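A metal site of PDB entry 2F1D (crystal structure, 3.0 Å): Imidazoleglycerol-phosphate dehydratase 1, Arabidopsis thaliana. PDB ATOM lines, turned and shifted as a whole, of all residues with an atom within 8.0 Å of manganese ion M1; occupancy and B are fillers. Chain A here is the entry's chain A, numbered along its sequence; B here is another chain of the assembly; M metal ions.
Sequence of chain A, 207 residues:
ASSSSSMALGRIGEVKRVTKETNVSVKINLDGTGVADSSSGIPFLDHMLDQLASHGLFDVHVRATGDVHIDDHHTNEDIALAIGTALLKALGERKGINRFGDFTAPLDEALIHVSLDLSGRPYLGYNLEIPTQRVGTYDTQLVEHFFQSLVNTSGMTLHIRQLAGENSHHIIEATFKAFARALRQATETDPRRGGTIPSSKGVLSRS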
ATOM      1  N   PHE A  44     -22.340   8.645  -2.385  1.00  0.00           N
ATOM      2  CA  PHE A  44     -21.479   7.675  -1.719  1.00  0.00           C
ATOM      3  C   PHE A  44     -21.010   8.177  -0.366  1.00  0.00           C
ATOM      4  O   PHE A  44     -20.904   7.380   0.558  1.00  0.00           O
ATOM      5  CB  PHE A  44     -20.262   7.276  -2.567  1.00  0.00           C
ATOM      6  CG  PHE A  44     -19.551   6.067  -2.022  1.00  0.00           C
ATOM      7  CD1 PHE A  44     -20.053   4.810  -2.271  1.00  0.00           C
ATOM      8  CD2 PHE A  44     -18.422   6.194  -1.238  1.00  0.00           C
ATOM      9  CE1 PHE A  44     -19.433   3.707  -1.774  1.00  0.00           C
ATOM     10  CE2 PHE A  44     -17.796   5.071  -0.718  1.00  0.00           C
ATOM     11  CZ  PHE A  44     -18.305   3.823  -0.989  1.00  0.00           C
ATOM     12  N   HIS A  47     -23.806   7.529   2.167  1.00  0.00           N
ATOM     13  CA  HIS A  47     -23.765   6.143   2.582  1.00  0.00           C
ATOM     14  C   HIS A  47     -22.703   5.949   3.640  1.00  0.00           C
ATOM     15  O   HIS A  47     -22.948   5.254   4.621  1.00  0.00           O
ATOM     16  CB  HIS A  47     -23.466   5.255   1.380  1.00  0.00           C
ATOM     17  CG  HIS A  47     -23.537   3.786   1.665  1.00  0.00           C
ATOM     18  ND1 HIS A  47     -24.631   3.197   2.254  1.00  0.00           N
ATOM     19  CD2 HIS A  47     -22.653   2.794   1.422  1.00  0.00           C
ATOM     20  CE1 HIS A  47     -24.421   1.895   2.369  1.00  0.00           C
ATOM     21  NE2 HIS A  47     -23.222   1.623   1.865  1.00  0.00           N
ATOM     22  N   MET A  48     -21.547   6.584   3.471  1.00  0.00           N
ATOM     23  CA  MET A  48     -20.420   6.389   4.371  1.00  0.00           C
ATOM     24  C   MET A  48     -20.659   7.060   5.697  1.00  0.00           C
ATOM     25  O   MET A  48     -20.257   6.547   6.731  1.00  0.00           O
ATOM     26  CB  MET A  48     -19.133   6.926   3.765  1.00  0.00           C
ATOM     27  CG  MET A  48     -18.513   5.975   2.761  1.00  0.00           C
ATOM     28  SD  MET A  48     -18.475   4.294   3.353  1.00  0.00           S
ATOM     29  CE  MET A  48     -19.693   3.620   2.455  1.00  0.00           C
ATOM     30  N   GLN A  51     -22.976   5.081   7.817  1.00  0.00           N
ATOM     31  CA  GLN A  51     -22.245   4.015   8.504  1.00  0.00           C
ATOM     32  C   GLN A  51     -21.527   4.552   9.750  1.00  0.00           C
ATOM     33  O   GLN A  51     -21.488   3.893  10.778  1.00  0.00           O
ATOM     34  CB  GLN A  51     -21.237   3.346   7.570  1.00  0.00           C
ATOM     35  CG  GLN A  51     -21.846   2.688   6.337  1.00  0.00           C
ATOM     36  CD  GLN A  51     -22.517   1.340   6.624  1.00  0.00           C
ATOM     37  OE1 GLN A  51     -21.926   0.455   7.258  1.00  0.00           O
ATOM     38  NE2 GLN A  51     -23.739   1.182   6.132  1.00  0.00           N
ATOM     39  N   LEU A 107     -15.211  -6.422   6.547  1.00  0.00           N
ATOM     40  CA  LEU A 107     -16.412  -6.553   5.738  1.00  0.00           C
ATOM     41  C   LEU A 107     -16.080  -7.481   4.575  1.00  0.00           C
ATOM     42  O   LEU A 107     -15.446  -7.076   3.598  1.00  0.00           O
ATOM     43  CB  LEU A 107     -16.899  -5.190   5.246  1.00  0.00           C
ATOM     44  CG  LEU A 107     -17.864  -5.111   4.052  1.00  0.00           C
ATOM     45  CD1 LEU A 107     -18.920  -6.174   4.079  1.00  0.00           C
ATOM     46  CD2 LEU A 107     -18.511  -3.734   4.042  1.00  0.00           C
ATOM     47  N   HIS A 169     -15.617  -0.928  -2.569  1.00  0.00           N
ATOM     48  CA  HIS A 169     -16.771  -0.520  -1.774  1.00  0.00           C
ATOM     49  C   HIS A 169     -16.681  -1.149  -0.389  1.00  0.00           C
ATOM     50  O   HIS A 169     -17.141  -0.561   0.585  1.00  0.00           O
ATOM     51  CB  HIS A 169     -18.070  -0.936  -2.494  1.00  0.00           C
ATOM     52  CG  HIS A 169     -19.333  -0.527  -1.787  1.00  0.00           C
ATOM     53  ND1 HIS A 169     -19.810   0.764  -1.789  1.00  0.00           N
ATOM     54  CD2 HIS A 169     -20.253  -1.255  -1.108  1.00  0.00           C
ATOM     55  CE1 HIS A 169     -20.948   0.824  -1.119  1.00  0.00           C
ATOM     56  NE2 HIS A 169     -21.230  -0.388  -0.692  1.00  0.00           N
ATOM     57  N   HIS A 170     -16.062  -2.325  -0.318  1.00  0.00           N
ATOM     58  CA  HIS A 170     -15.857  -3.038   0.942  1.00  0.00           C
ATOM     59  C   HIS A 170     -14.717  -2.475   1.762  1.00  0.00           C
ATOM     60  O   HIS A 170     -14.767  -2.540   2.979  1.00  0.00           O
ATOM     61  CB  HIS A 170     -15.520  -4.492   0.681  1.00  0.00           C
ATOM     62  CG  HIS A 170     -16.700  -5.320   0.301  1.00  0.00           C
ATOM     63  ND1 HIS A 170     -16.587  -6.647  -0.025  1.00  0.00           N
ATOM     64  CD2 HIS A 170     -18.002  -5.009   0.180  1.00  0.00           C
ATOM     65  CE1 HIS A 170     -17.778  -7.131  -0.317  1.00  0.00           C
ATOM     66  NE2 HIS A 170     -18.661  -6.153  -0.207  1.00  0.00           N
ATOM     67  N   GLU A 173     -15.861   1.049   3.134  1.00  0.00           N
ATOM     68  CA  GLU A 173     -16.932   0.890   4.100  1.00  0.00           C
ATOM     69  C   GLU A 173     -16.442   0.307   5.434  1.00  0.00           C
ATOM     70  O   GLU A 173     -16.866   0.720   6.516  1.00  0.00           O
ATOM     71  CB  GLU A 173     -18.007  -0.010   3.515  1.00  0.00           C
ATOM     72  CG  GLU A 173     -19.234  -0.202   4.399  1.00  0.00           C
ATOM     73  CD  GLU A 173     -20.500  -0.346   3.602  1.00  0.00           C
ATOM     74  OE1 GLU A 173     -20.505   0.009   2.402  1.00  0.00           O
ATOM     75  OE2 GLU A 173     -21.496  -0.814   4.188  1.00  0.00           O
ATOM     76  N   LYS A 177     -16.618   1.847   9.249  1.00  0.00           N
ATOM     77  CA  LYS A 177     -17.147   1.050  10.344  1.00  0.00           C
ATOM     78  C   LYS A 177     -16.155   1.035  11.495  1.00  0.00           C
ATOM     79  O   LYS A 177     -16.538   1.148  12.646  1.00  0.00           O
ATOM     80  CB  LYS A 177     -17.433  -0.389   9.904  1.00  0.00           C
ATOM     81  CG  LYS A 177     -18.735  -0.555   9.160  1.00  0.00           C
ATOM     82  CD  LYS A 177     -18.972  -1.991   8.696  1.00  0.00           C
ATOM     83  CE  LYS A 177     -20.226  -2.063   7.827  1.00  0.00           C
ATOM     84  NZ  LYS A 177     -20.471  -3.369   7.138  1.00  0.00           N
ATOM     85  N   GLU B  21     -32.189  -1.376   1.534  1.00  0.00           N
ATOM     86  CA  GLU B  21     -31.542  -0.907   0.309  1.00  0.00           C
ATOM     87  C   GLU B  21     -32.288  -1.285  -0.994  1.00  0.00           C
ATOM     88  O   GLU B  21     -32.519  -0.417  -1.842  1.00  0.00           O
ATOM     89  CB  GLU B  21     -30.104  -1.430   0.266  1.00  0.00           C
ATOM     90  CG  GLU B  21     -29.154  -0.683   1.219  1.00  0.00           C
ATOM     91  CD  GLU B  21     -28.486  -1.586   2.256  1.00  0.00           C
ATOM     92  OE1 GLU B  21     -29.177  -2.460   2.818  1.00  0.00           O
ATOM     93  OE2 GLU B  21     -27.270  -1.399   2.518  1.00  0.00           O
ATOM     94  N   ASP B  67     -30.308   1.096  -4.587  1.00  0.00           N
ATOM     95  CA  ASP B  67     -29.454   2.286  -4.455  1.00  0.00           C
ATOM     96  C   ASP B  67     -28.701   2.701  -5.708  1.00  0.00           C
ATOM     97  O   ASP B  67     -27.655   3.344  -5.596  1.00  0.00           O
ATOM     98  CB  ASP B  67     -28.318   2.070  -3.447  1.00  0.00           C
ATOM     99  CG  ASP B  67     -28.764   1.463  -2.189  1.00  0.00           C
ATOM    100  OD1 ASP B  67     -28.865   2.209  -1.189  1.00  0.00           O
ATOM    101  OD2 ASP B  67     -28.945   0.238  -2.092  1.00  0.00           O
ATOM    102  N   ILE B  70     -26.203   5.637  -5.452  1.00  0.00           N
ATOM    103  CA  ILE B  70     -24.908   5.536  -4.747  1.00  0.00           C
ATOM    104  C   ILE B  70     -23.915   4.775  -5.607  1.00  0.00           C
ATOM    105  O   ILE B  70     -22.943   5.333  -6.123  1.00  0.00           O
ATOM    106  CB  ILE B  70     -24.994   4.739  -3.409  1.00  0.00           C
ATOM    107  CG1 ILE B  70     -25.993   5.333  -2.411  1.00  0.00           C
ATOM    108  CG2 ILE B  70     -23.612   4.631  -2.799  1.00  0.00           C
ATOM    109  CD1 ILE B  70     -26.330   4.381  -1.260  1.00  0.00           C
ATOM    110  N   ASP B  71     -24.226   3.477  -5.768  1.00  0.00           N
ATOM    111  CA  ASP B  71     -23.357   2.429  -6.290  1.00  0.00           C
ATOM    112  C   ASP B  71     -24.248   1.534  -7.146  1.00  0.00           C
ATOM    113  O   ASP B  71     -25.437   1.765  -7.243  1.00  0.00           O
ATOM    114  CB  ASP B  71     -22.862   1.598  -5.110  1.00  0.00           C
ATOM    115  CG  ASP B  71     -21.430   1.187  -5.248  1.00  0.00           C
ATOM    116  OD1 ASP B  71     -20.806   1.507  -6.274  1.00  0.00           O
ATOM    117  OD2 ASP B  71     -20.827   0.539  -4.360  1.00  0.00           O
ATOM    118  N   HIS B  73     -23.496  -1.637  -6.281  1.00  0.00           N
ATOM    119  CA  HIS B  73     -23.067  -2.733  -5.399  1.00  0.00           C
ATOM    120  C   HIS B  73     -24.185  -3.474  -4.639  1.00  0.00           C
ATOM    121  O   HIS B  73     -24.188  -4.691  -4.586  1.00  0.00           O
ATOM    122  CB  HIS B  73     -22.045  -2.200  -4.393  1.00  0.00           C
ATOM    123  CG  HIS B  73     -21.340  -3.275  -3.619  1.00  0.00           C
ATOM    124  ND1 HIS B  73     -20.081  -3.708  -3.953  1.00  0.00           N
ATOM    125  CD2 HIS B  73     -21.728  -4.008  -2.557  1.00  0.00           C
ATOM    126  CE1 HIS B  73     -19.725  -4.669  -3.110  1.00  0.00           C
ATOM    127  NE2 HIS B  73     -20.704  -4.859  -2.259  1.00  0.00           N
ATOM    128  N   HIS B  74     -25.081  -2.717  -4.031  1.00  0.00           N
ATOM    129  CA  HIS B  74     -26.132  -3.264  -3.178  1.00  0.00           C
ATOM    130  C   HIS B  74     -27.191  -4.022  -3.954  1.00  0.00           C
ATOM    131  O   HIS B  74     -27.700  -5.036  -3.487  1.00  0.00           O
ATOM    132  CB  HIS B  74     -26.823  -2.158  -2.407  1.00  0.00           C
ATOM    133  CG  HIS B  74     -25.938  -1.433  -1.441  1.00  0.00           C
ATOM    134  ND1 HIS B  74     -26.240  -0.183  -0.957  1.00  0.00           N
ATOM    135  CD2 HIS B  74     -24.767  -1.787  -0.870  1.00  0.00           C
ATOM    136  CE1 HIS B  74     -25.288   0.208  -0.127  1.00  0.00           C
ATOM    137  NE2 HIS B  74     -24.382  -0.745  -0.055  1.00  0.00           N
ATOM    138  N   GLU B  77     -25.677  -7.371  -5.416  1.00  0.00           N
ATOM    139  CA  GLU B  77     -25.483  -8.434  -4.442  1.00  0.00           C
ATOM    140  C   GLU B  77     -26.813  -9.008  -3.937  1.00  0.00           C
ATOM    141  O   GLU B  77     -26.926 -10.220  -3.752  1.00  0.00           O
ATOM    142  CB  GLU B  77     -24.628  -7.927  -3.256  1.00  0.00           C
ATOM    143  CG  GLU B  77     -24.920  -8.644  -1.930  1.00  0.00           C
ATOM    144  CD  GLU B  77     -23.856  -8.405  -0.884  1.00  0.00           C
ATOM    145  OE1 GLU B  77     -23.152  -7.362  -0.958  1.00  0.00           O
ATOM    146  OE2 GLU B  77     -23.729  -9.267   0.017  1.00  0.00           O
HETATM  147 MN    MN M   1     -22.656  -0.573   1.380  1.00  0.00          MN
HETATM  148 MN    MN M   2     -20.960  -6.672  -0.539  1.00  0.00          MN
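The side-chain amide oxygen (OE1) of Gln 51 lies close to the side-chain carboxylate (OE2) of Glu 173 (3.3 Å).
ND1 of His 74 of chain B is in hydrogen-bond range of OD2 of Asp 67 of chain B, at 3.0 Å.
ND1 of His 169 is in hydrogen-bond range of OD2 of Asp 71 of chain B, 2.8 Å away.
Of the 16 residues printed, 4 come within 4 Å of manganese ion M1.
The nearest printed residue that does not touch manganese ion M1 is Glu 21 of chain B (4.8 Å).
Manganese ion M1 is bound by a ring nitrogen (NE2) of His 74 of chain B (2.3 Å), a ring nitrogen (NE2) of His 47 (2.3 Å), the side-chain carboxylate (OE1) of Glu 173 (2.5 Å) and a ring nitrogen (NE2) of His 169 (2.5 Å).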
